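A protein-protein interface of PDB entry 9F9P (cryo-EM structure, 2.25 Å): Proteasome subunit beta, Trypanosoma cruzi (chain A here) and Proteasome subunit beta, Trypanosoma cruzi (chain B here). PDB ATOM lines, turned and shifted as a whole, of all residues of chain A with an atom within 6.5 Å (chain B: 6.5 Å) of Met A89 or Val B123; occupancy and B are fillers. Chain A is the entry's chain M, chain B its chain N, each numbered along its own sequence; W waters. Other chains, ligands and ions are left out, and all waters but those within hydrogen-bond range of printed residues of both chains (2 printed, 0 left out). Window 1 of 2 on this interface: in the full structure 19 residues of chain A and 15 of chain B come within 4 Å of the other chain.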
ATOM      1  N   TRP A  33     -30.887   4.229  13.398  1.00  0.00           N
ATOM      2  CA  TRP A  33     -29.559   3.593  13.624  1.00  0.00           C
ATOM      3  C   TRP A  33     -29.030   4.044  14.976  1.00  0.00           C
ATOM      4  O   TRP A  33     -28.988   5.238  15.265  1.00  0.00           O
ATOM      5  CB  TRP A  33     -28.560   3.934  12.503  1.00  0.00           C
ATOM      6  CG  TRP A  33     -27.235   3.236  12.638  1.00  0.00           C
ATOM      7  CD1 TRP A  33     -26.912   1.954  12.264  1.00  0.00           C
ATOM      8  CD2 TRP A  33     -26.060   3.775  13.279  1.00  0.00           C
ATOM      9  NE1 TRP A  33     -25.603   1.681  12.582  1.00  0.00           N
ATOM     10  CE2 TRP A  33     -25.063   2.774  13.222  1.00  0.00           C
ATOM     11  CE3 TRP A  33     -25.758   5.016  13.847  1.00  0.00           C
ATOM     12  CZ2 TRP A  33     -23.773   2.996  13.693  1.00  0.00           C
ATOM     13  CZ3 TRP A  33     -24.489   5.228  14.352  1.00  0.00           C
ATOM     14  CH2 TRP A  33     -23.507   4.227  14.270  1.00  0.00           C
ATOM     15  N   SER A  34     -28.616   3.065  15.781  1.00  0.00           N
ATOM     16  CA  SER A  34     -27.881   3.328  17.008  1.00  0.00           C
ATOM     17  C   SER A  34     -26.483   2.736  16.861  1.00  0.00           C
ATOM     18  O   SER A  34     -26.271   1.757  16.162  1.00  0.00           O
ATOM     19  CB  SER A  34     -28.590   2.752  18.220  1.00  0.00           C
ATOM     20  OG  SER A  34     -27.765   2.855  19.381  1.00  0.00           O
ATOM     21  N   PRO A  35     -25.474   3.325  17.503  1.00  0.00           N
ATOM     22  CA  PRO A  35     -24.176   2.665  17.599  1.00  0.00           C
ATOM     23  C   PRO A  35     -24.077   1.545  18.652  1.00  0.00           C
ATOM     24  O   PRO A  35     -23.007   0.960  18.813  1.00  0.00           O
ATOM     25  CB  PRO A  35     -23.266   3.858  17.930  1.00  0.00           C
ATOM     26  CG  PRO A  35     -24.155   4.759  18.775  1.00  0.00           C
ATOM     27  CD  PRO A  35     -25.507   4.671  18.088  1.00  0.00           C
ATOM     28  N   TYR A  36     -25.198   1.214  19.323  1.00  0.00           N
ATOM     29  CA  TYR A  36     -25.199   0.203  20.376  1.00  0.00           C
ATOM     30  C   TYR A  36     -26.115  -0.968  20.006  1.00  0.00           C
ATOM     31  O   TYR A  36     -27.142  -0.773  19.377  1.00  0.00           O
ATOM     32  CB  TYR A  36     -25.583   0.828  21.722  1.00  0.00           C
ATOM     33  CG  TYR A  36     -24.582   1.822  22.263  1.00  0.00           C
ATOM     34  CD1 TYR A  36     -23.257   1.462  22.461  1.00  0.00           C
ATOM     35  CD2 TYR A  36     -24.932   3.130  22.559  1.00  0.00           C
ATOM     36  CE1 TYR A  36     -22.312   2.358  22.945  1.00  0.00           C
ATOM     37  CE2 TYR A  36     -23.992   4.051  23.016  1.00  0.00           C
ATOM     38  CZ  TYR A  36     -22.685   3.655  23.247  1.00  0.00           C
ATOM     39  OH  TYR A  36     -21.728   4.513  23.776  1.00  0.00           O
ATOM     40  N   ALA A  37     -25.685  -2.186  20.376  1.00  0.00           N
ATOM     41  CA  ALA A  37     -26.464  -3.419  20.302  1.00  0.00           C
ATOM     42  C   ALA A  37     -26.141  -4.262  21.544  1.00  0.00           C
ATOM     43  O   ALA A  37     -24.972  -4.291  21.948  1.00  0.00           O
ATOM     44  CB  ALA A  37     -26.109  -4.158  19.028  1.00  0.00           C
ATOM     45  N   ASP A  38     -27.142  -4.891  22.183  1.00  0.00           N
ATOM     46  CA  ASP A  38     -26.893  -5.863  23.245  1.00  0.00           C
ATOM     47  C   ASP A  38     -26.951  -7.285  22.682  1.00  0.00           C
ATOM     48  O   ASP A  38     -27.996  -7.724  22.211  1.00  0.00           O
ATOM     49  CB  ASP A  38     -27.890  -5.767  24.410  1.00  0.00           C
ATOM     50  CG  ASP A  38     -27.502  -6.555  25.679  1.00  0.00           C
ATOM     51  OD1 ASP A  38     -26.551  -7.384  25.633  1.00  0.00           O
ATOM     52  OD2 ASP A  38     -28.136  -6.322  26.743  1.00  0.00           O
ATOM     53  N   ASN A  39     -25.843  -8.020  22.761  1.00  0.00           N
ATOM     54  CA  ASN A  39     -25.793  -9.361  22.180  1.00  0.00           C
ATOM     55  C   ASN A  39     -26.095 -10.442  23.202  1.00  0.00           C
ATOM     56  O   ASN A  39     -26.128 -11.628  22.858  1.00  0.00           O
ATOM     57  CB  ASN A  39     -24.468  -9.596  21.450  1.00  0.00           C
ATOM     58  CG  ASN A  39     -24.281  -8.648  20.275  1.00  0.00           C
ATOM     59  OD1 ASN A  39     -23.438  -7.753  20.269  1.00  0.00           O
ATOM     60  ND2 ASN A  39     -25.118  -8.823  19.283  1.00  0.00           N
ATOM     61  N   GLY A  40     -26.324 -10.078  24.462  1.00  0.00           N
ATOM     62  CA  GLY A  40     -26.824 -11.065  25.419  1.00  0.00           C
ATOM     63  C   GLY A  40     -25.765 -11.968  26.085  1.00  0.00           C
ATOM     64  O   GLY A  40     -24.574 -11.899  25.818  1.00  0.00           O
ATOM     65  N   THR A  87     -19.488  -9.001  28.868  1.00  0.00           N
ATOM     66  CA  THR A  87     -20.833  -9.145  28.339  1.00  0.00           C
ATOM     67  C   THR A  87     -21.316  -7.809  27.815  1.00  0.00           C
ATOM     68  O   THR A  87     -20.745  -6.777  28.109  1.00  0.00           O
ATOM     69  CB  THR A  87     -21.892  -9.580  29.382  1.00  0.00           C
ATOM     70  OG1 THR A  87     -22.022  -8.685  30.507  1.00  0.00           O
ATOM     71  CG2 THR A  87     -21.585 -10.926  29.974  1.00  0.00           C
ATOM     72  N   GLY A  88     -22.381  -7.817  27.041  1.00  0.00           N
ATOM     73  CA  GLY A  88     -22.842  -6.574  26.457  1.00  0.00           C
ATOM     74  C   GLY A  88     -22.763  -6.624  24.945  1.00  0.00           C
ATOM     75  O   GLY A  88     -23.169  -7.628  24.340  1.00  0.00           O
ATOM     76  N   MET A  89     -22.140  -5.606  24.367  1.00  0.00           N
ATOM     77  CA  MET A  89     -21.984  -5.528  22.918  1.00  0.00           C
ATOM     78  C   MET A  89     -20.729  -6.256  22.461  1.00  0.00           C
ATOM     79  O   MET A  89     -19.646  -5.953  22.903  1.00  0.00           O
ATOM     80  CB  MET A  89     -21.886  -4.058  22.548  1.00  0.00           C
ATOM     81  CG  MET A  89     -21.850  -3.829  21.099  1.00  0.00           C
ATOM     82  SD  MET A  89     -21.923  -2.060  20.760  1.00  0.00           S
ATOM     83  CE  MET A  89     -21.640  -2.178  19.004  1.00  0.00           C
ATOM     84  N   GLN A  90     -20.854  -7.204  21.564  1.00  0.00           N
ATOM     85  CA  GLN A  90     -19.724  -7.986  21.116  1.00  0.00           C
ATOM     86  C   GLN A  90     -18.681  -7.161  20.367  1.00  0.00           C
ATOM     87  O   GLN A  90     -17.511  -7.463  20.492  1.00  0.00           O
ATOM     88  CB  GLN A  90     -20.167  -9.101  20.169  1.00  0.00           C
ATOM     89  CG  GLN A  90     -19.072 -10.107  19.865  1.00  0.00           C
ATOM     90  CD  GLN A  90     -18.931 -10.439  18.406  1.00  0.00           C
ATOM     91  OE1 GLN A  90     -19.086  -9.613  17.540  1.00  0.00           O
ATOM     92  NE2 GLN A  90     -18.644 -11.678  18.113  1.00  0.00           N
ATOM     93  N   ALA A  91     -19.036  -6.132  19.616  1.00  0.00           N
ATOM     94  CA  ALA A  91     -18.011  -5.404  18.870  1.00  0.00           C
ATOM     95  C   ALA A  91     -17.112  -4.592  19.804  1.00  0.00           C
ATOM     96  O   ALA A  91     -15.938  -4.412  19.503  1.00  0.00           O
ATOM     97  CB  ALA A  91     -18.594  -4.491  17.801  1.00  0.00           C
ATOM     98  N   ASP A  92     -17.653  -4.120  20.921  1.00  0.00           N
ATOM     99  CA  ASP A  92     -16.882  -3.358  21.903  1.00  0.00           C
ATOM    100  C   ASP A  92     -15.957  -4.231  22.726  1.00  0.00           C
ATOM    101  O   ASP A  92     -14.865  -3.815  22.995  1.00  0.00           O
ATOM    102  CB  ASP A  92     -17.805  -2.546  22.804  1.00  0.00           C
ATOM    103  CG  ASP A  92     -18.159  -1.205  22.194  1.00  0.00           C
ATOM    104  OD1 ASP A  92     -17.601  -0.880  21.093  1.00  0.00           O
ATOM    105  OD2 ASP A  92     -18.897  -0.419  22.848  1.00  0.00           O
ATOM    106  N   ARG A  93     -16.366  -5.445  23.111  1.00  0.00           N
ATOM    107  CA  ARG A  93     -15.394  -6.311  23.751  1.00  0.00           C
ATOM    108  C   ARG A  93     -14.275  -6.738  22.796  1.00  0.00           C
ATOM    109  O   ARG A  93     -13.150  -6.848  23.230  1.00  0.00           O
ATOM    110  CB  ARG A  93     -15.987  -7.498  24.514  1.00  0.00           C
ATOM    111  CG  ARG A  93     -16.760  -8.497  23.681  1.00  0.00           C
ATOM    112  CD  ARG A  93     -17.051  -9.790  24.453  1.00  0.00           C
ATOM    113  NE  ARG A  93     -17.813 -10.759  23.692  1.00  0.00           N
ATOM    114  CZ  ARG A  93     -19.138 -10.801  23.665  1.00  0.00           C
ATOM    115  NH1 ARG A  93     -19.708 -11.788  23.010  1.00  0.00           N
ATOM    116  NH2 ARG A  93     -19.903  -9.927  24.304  1.00  0.00           N
ATOM    117  N   LEU A  94     -14.523  -6.910  21.515  1.00  0.00           N
ATOM    118  CA  LEU A  94     -13.434  -7.161  20.585  1.00  0.00           C
ATOM    119  C   LEU A  94     -12.407  -6.020  20.543  1.00  0.00           C
ATOM    120  O   LEU A  94     -11.223  -6.295  20.467  1.00  0.00           O
ATOM    121  CB  LEU A  94     -13.980  -7.410  19.186  1.00  0.00           C
ATOM    122  CG  LEU A  94     -14.759  -8.700  19.030  1.00  0.00           C
ATOM    123  CD1 LEU A  94     -15.179  -8.907  17.583  1.00  0.00           C
ATOM    124  CD2 LEU A  94     -14.010  -9.919  19.499  1.00  0.00           C
ATOM    125  N   TYR A 138     -19.730  -0.229  25.570  1.00  0.00           N
ATOM    126  CA  TYR A 138     -20.937  -0.810  26.137  1.00  0.00           C
ATOM    127  C   TYR A 138     -20.653  -2.255  26.565  1.00  0.00           C
ATOM    128  O   TYR A 138     -20.982  -3.190  25.859  1.00  0.00           O
ATOM    129  CB  TYR A 138     -22.112  -0.659  25.165  1.00  0.00           C
ATOM    130  CG  TYR A 138     -23.431  -1.168  25.696  1.00  0.00           C
ATOM    131  CD1 TYR A 138     -23.763  -1.046  27.038  1.00  0.00           C
ATOM    132  CD2 TYR A 138     -24.371  -1.745  24.855  1.00  0.00           C
ATOM    133  CE1 TYR A 138     -24.972  -1.512  27.533  1.00  0.00           C
ATOM    134  CE2 TYR A 138     -25.586  -2.213  25.332  1.00  0.00           C
ATOM    135  CZ  TYR A 138     -25.886  -2.100  26.677  1.00  0.00           C
ATOM    136  OH  TYR A 138     -27.089  -2.557  27.165  1.00  0.00           O
ATOM    137  N   THR A 139     -19.964  -2.407  27.695  1.00  0.00           N
ATOM    138  CA  THR A 139     -19.431  -3.681  28.136  1.00  0.00           C
ATOM    139  C   THR A 139     -19.530  -3.809  29.654  1.00  0.00           C
ATOM    140  O   THR A 139     -19.297  -2.847  30.377  1.00  0.00           O
ATOM    141  CB  THR A 139     -17.936  -3.862  27.794  1.00  0.00           C
ATOM    142  OG1 THR A 139     -17.177  -2.772  28.335  1.00  0.00           O
ATOM    143  CG2 THR A 139     -17.629  -4.014  26.317  1.00  0.00           C
ATOM    144  N   PHE A 140     -19.768  -5.020  30.155  1.00  0.00           N
ATOM    145  CA  PHE A 140     -19.641  -5.291  31.577  1.00  0.00           C
ATOM    146  C   PHE A 140     -18.518  -6.287  31.727  1.00  0.00           C
ATOM    147  O   PHE A 140     -18.676  -7.406  31.297  1.00  0.00           O
ATOM    148  CB  PHE A 140     -20.978  -5.795  32.125  1.00  0.00           C
ATOM    149  CG  PHE A 140     -22.058  -4.751  32.089  1.00  0.00           C
ATOM    150  CD1 PHE A 140     -22.180  -3.825  33.120  1.00  0.00           C
ATOM    151  CD2 PHE A 140     -22.845  -4.592  30.951  1.00  0.00           C
ATOM    152  CE1 PHE A 140     -23.116  -2.799  33.039  1.00  0.00           C
ATOM    153  CE2 PHE A 140     -23.774  -3.558  30.868  1.00  0.00           C
ATOM    154  CZ  PHE A 140     -23.907  -2.665  31.913  1.00  0.00           C
ATOM    155  N   GLN B  88     -14.125  -6.115   8.879  1.00  0.00           N
ATOM    156  CA  GLN B  88     -14.695  -5.847  10.188  1.00  0.00           C
ATOM    157  C   GLN B  88     -14.076  -4.643  10.900  1.00  0.00           C
ATOM    158  O   GLN B  88     -14.794  -3.913  11.544  1.00  0.00           O
ATOM    159  CB  GLN B  88     -14.633  -7.079  11.088  1.00  0.00           C
ATOM    160  CG  GLN B  88     -15.407  -6.892  12.400  1.00  0.00           C
ATOM    161  CD  GLN B  88     -14.652  -6.297  13.574  1.00  0.00           C
ATOM    162  OE1 GLN B  88     -13.423  -6.352  13.672  1.00  0.00           O
ATOM    163  NE2 GLN B  88     -15.394  -5.750  14.521  1.00  0.00           N
ATOM    164  N   VAL B  91     -15.610  -1.405   9.146  1.00  0.00           N
ATOM    165  CA  VAL B  91     -16.989  -1.190   9.589  1.00  0.00           C
ATOM    166  C   VAL B  91     -17.029  -0.662  11.020  1.00  0.00           C
ATOM    167  O   VAL B  91     -17.762   0.257  11.297  1.00  0.00           O
ATOM    168  CB  VAL B  91     -17.798  -2.504   9.459  1.00  0.00           C
ATOM    169  CG1 VAL B  91     -19.172  -2.436  10.114  1.00  0.00           C
ATOM    170  CG2 VAL B  91     -17.961  -2.977   8.020  1.00  0.00           C
ATOM    171  N   TYR B  92     -16.253  -1.205  11.939  1.00  0.00           N
ATOM    172  CA  TYR B  92     -16.248  -0.699  13.308  1.00  0.00           C
ATOM    173  C   TYR B  92     -15.717   0.726  13.419  1.00  0.00           C
ATOM    174  O   TYR B  92     -16.235   1.510  14.186  1.00  0.00           O
ATOM    175  CB  TYR B  92     -15.417  -1.596  14.228  1.00  0.00           C
ATOM    176  CG  TYR B  92     -15.413  -1.205  15.689  1.00  0.00           C
ATOM    177  CD1 TYR B  92     -16.535  -1.428  16.468  1.00  0.00           C
ATOM    178  CD2 TYR B  92     -14.358  -0.522  16.272  1.00  0.00           C
ATOM    179  CE1 TYR B  92     -16.570  -1.076  17.797  1.00  0.00           C
ATOM    180  CE2 TYR B  92     -14.404  -0.117  17.598  1.00  0.00           C
ATOM    181  CZ  TYR B  92     -15.492  -0.436  18.372  1.00  0.00           C
ATOM    182  OH  TYR B  92     -15.647  -0.106  19.680  1.00  0.00           O
ATOM    183  N   ARG B  95     -18.475   3.095  12.282  1.00  0.00           N
ATOM    184  CA  ARG B  95     -19.467   3.172  13.362  1.00  0.00           C
ATOM    185  C   ARG B  95     -19.008   4.123  14.459  1.00  0.00           C
ATOM    186  O   ARG B  95     -19.806   4.838  15.008  1.00  0.00           O
ATOM    187  CB  ARG B  95     -19.707   1.769  13.928  1.00  0.00           C
ATOM    188  CG  ARG B  95     -20.551   1.683  15.190  1.00  0.00           C
ATOM    189  CD  ARG B  95     -19.659   1.517  16.384  1.00  0.00           C
ATOM    190  NE  ARG B  95     -20.344   1.542  17.647  1.00  0.00           N
ATOM    191  CZ  ARG B  95     -19.740   1.582  18.824  1.00  0.00           C
ATOM    192  NH1 ARG B  95     -18.447   1.803  18.918  1.00  0.00           N
ATOM    193  NH2 ARG B  95     -20.454   1.441  19.918  1.00  0.00           N
ATOM    194  N   CYS B 101     -21.401   2.305   7.834  1.00  0.00           N
ATOM    195  CA  CYS B 101     -21.650   1.539   6.618  1.00  0.00           C
ATOM    196  C   CYS B 101     -22.986   0.792   6.744  1.00  0.00           C
ATOM    197  O   CYS B 101     -23.021  -0.239   7.422  1.00  0.00           O
ATOM    198  CB  CYS B 101     -20.490   0.559   6.405  1.00  0.00           C
ATOM    199  SG  CYS B 101     -20.546  -0.315   4.808  1.00  0.00           S
ATOM    200  N   CYS B 103     -24.991  -1.575   5.776  1.00  0.00           N
ATOM    201  CA  CYS B 103     -25.112  -2.857   5.121  1.00  0.00           C
ATOM    202  C   CYS B 103     -24.891  -3.965   6.129  1.00  0.00           C
ATOM    203  O   CYS B 103     -24.210  -3.776   7.110  1.00  0.00           O
ATOM    204  CB  CYS B 103     -23.921  -3.184   4.240  1.00  0.00           C
ATOM    205  SG  CYS B 103     -23.754  -2.146   2.801  1.00  0.00           S
ATOM    206  N   VAL B 120     -20.905  -9.953   9.012  1.00  0.00           N
ATOM    207  CA  VAL B 120     -20.570  -8.738   9.732  1.00  0.00           C
ATOM    208  C   VAL B 120     -21.759  -7.788   9.684  1.00  0.00           C
ATOM    209  O   VAL B 120     -22.176  -7.440   8.601  1.00  0.00           O
ATOM    210  CB  VAL B 120     -19.369  -7.991   9.107  1.00  0.00           C
ATOM    211  CG1 VAL B 120     -19.000  -6.761   9.925  1.00  0.00           C
ATOM    212  CG2 VAL B 120     -18.139  -8.829   8.963  1.00  0.00           C
ATOM    213  N   ASP B 121     -22.195  -7.228  10.815  1.00  0.00           N
ATOM    214  CA  ASP B 121     -23.288  -6.260  10.770  1.00  0.00           C
ATOM    215  C   ASP B 121     -22.774  -4.836  10.872  1.00  0.00           C
ATOM    216  O   ASP B 121     -21.584  -4.617  11.092  1.00  0.00           O
ATOM    217  CB  ASP B 121     -24.356  -6.577  11.807  1.00  0.00           C
ATOM    218  CG  ASP B 121     -24.126  -6.080  13.222  1.00  0.00           C
ATOM    219  OD1 ASP B 121     -23.092  -5.417  13.515  1.00  0.00           O
ATOM    220  OD2 ASP B 121     -24.999  -6.389  14.088  1.00  0.00           O
ATOM    221  N   ASP B 122     -23.692  -3.871  10.823  1.00  0.00           N
ATOM    222  CA  ASP B 122     -23.327  -2.473  10.633  1.00  0.00           C
ATOM    223  C   ASP B 122     -22.845  -1.786  11.902  1.00  0.00           C
ATOM    224  O   ASP B 122     -22.503  -0.596  11.840  1.00  0.00           O
ATOM    225  CB  ASP B 122     -24.443  -1.648   9.987  1.00  0.00           C
ATOM    226  CG  ASP B 122     -25.714  -1.461  10.807  1.00  0.00           C
ATOM    227  OD1 ASP B 122     -26.767  -1.081  10.186  1.00  0.00           O
ATOM    228  OD2 ASP B 122     -25.685  -1.696  12.059  1.00  0.00           O
ATOM    229  N   VAL B 123     -22.807  -2.479  13.042  1.00  0.00           N
ATOM    230  CA  VAL B 123     -22.071  -1.917  14.157  1.00  0.00           C
ATOM    231  C   VAL B 123     -20.729  -2.627  14.364  1.00  0.00           C
ATOM    232  O   VAL B 123     -19.909  -2.171  15.146  1.00  0.00           O
ATOM    233  CB  VAL B 123     -22.925  -1.867  15.439  1.00  0.00           C
ATOM    234  CG1 VAL B 123     -24.122  -0.967  15.231  1.00  0.00           C
ATOM    235  CG2 VAL B 123     -23.375  -3.239  15.924  1.00  0.00           C
ATOM    236  N   GLY B 124     -20.487  -3.706  13.617  1.00  0.00           N
ATOM    237  CA  GLY B 124     -19.195  -4.385  13.614  1.00  0.00           C
ATOM    238  C   GLY B 124     -19.246  -5.751  14.289  1.00  0.00           C
ATOM    239  O   GLY B 124     -18.203  -6.290  14.562  1.00  0.00           O
ATOM    240  N   THR B 125     -20.435  -6.293  14.555  1.00  0.00           N
ATOM    241  CA  THR B 125     -20.583  -7.609  15.165  1.00  0.00           C
ATOM    242  C   THR B 125     -20.088  -8.629  14.143  1.00  0.00           C
ATOM    243  O   THR B 125     -20.396  -8.480  12.994  1.00  0.00           O
ATOM    244  CB  THR B 125     -22.069  -7.889  15.513  1.00  0.00           C
ATOM    245  OG1 THR B 125     -22.605  -6.784  16.230  1.00  0.00           O
ATOM    246  CG2 THR B 125     -22.290  -9.188  16.277  1.00  0.00           C
HETATM  247  O   HOH W   1     -14.585  -4.314  17.063  1.00  0.00           O
HETATM  248  O   HOH W   2     -21.863  -5.963  18.462  1.00  0.00           O
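The guanidinium group of Arg B95 lies within salt-bridge range of the side-chain carboxylate of Asp A92 (3.6 Å). The side-chain hydroxyl (OH) of Tyr B92 is in hydrogen-bond range of the side-chain carboxylate (OD1) of Asp A92 (2.5 Å). The guanidinium group of Arg B95 is in hydrogen-bond range of the backbone carbonyl oxygen of Pro A35, 2.8 Å away. NE1 of Trp A33 is in hydrogen-bond range of OD2 of Asp B122, at 3.4 Å.
OD1 of Asp B121 is in hydrogen-bond range of N of Val B123. The backbone NH (N) of Gln A90 lies within hydrogen-bond range of the side-chain amide oxygen (OD1) of Asn A39 (2.9 Å). OH of Tyr B92 sits at hydrogen-bond distance from NH1 of Arg B95, at 3.5 Å. OD1 of Asp B121 is in hydrogen-bond range of N of Thr B125, 3.0 Å away. The backbone NH (N) of Tyr A138 is in hydrogen-bond range of the side-chain carboxylate (OD2) of Asp A92, 2.9 Å away. N of Met A89 lies within hydrogen-bond range of O of Tyr A138, at 3.1 Å.
Among the printed residues, pairs that only touch across the chains: Gln A90 with Thr B125 (3.4 Å), Ser A34 with Val B123 (3.6 Å), Tyr A36 with Arg B95 (3.7 Å), Met A89 with Val B123 (3.7 Å), Ala A91 with Gly B124 (3.7 Å), Ala A91 with Val B123 (3.8 Å), Trp A33 with Arg B95 (3.8 Å), Ala A91 with Tyr B92 (3.8 Å) and Met A89 with Arg B95 (3.9 Å).
Of the printed residues of chain B, Ser A34 touches Val B123 (3.6 Å). Of the printed residues of chain B, Pro A35 touches Arg B95 (2.8 Å). Met A89 touches two residues of chain B. Printed residues of chain B within 4 Å of Ala A91: Tyr B92 (3.8 Å), Val B123 (3.8 Å) and Gly B124 (3.7 Å). Of the printed residues of chain A, Asp B122 touches Trp A33 (3.4 Å). Val B123 touches just these residues of chain A: Ser A34 (3.6 Å), Met A89 (3.7 Å) and Ala A91 (3.8 Å). Of the printed residues of chain A, Gly B124 touches Ala A91 (3.7 Å). The nearest residue of chain B that does not touch Met A89 is Tyr B92 (5.3 Å). The nearest residue of chain A that does not touch Val B123 is Trp A33 (4.03 Å).
Of the 19 printed residues of chain A, 8 touch a printed residue of chain B. Among the printed residues, 13 pairs touch across the chains.
Water W2 lies within hydrogen-bond range of the side-chain hydroxyl of Thr B125, the side-chain amide oxygen of Asn A39, the backbone NH of Ala A91 and the backbone NH of Gln A90. Water W1 bridges the backbone carbonyl oxygen of Ala A91 (2.8 Å) and the side-chain amide nitrogen of Gln B88 (3.0 Å).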
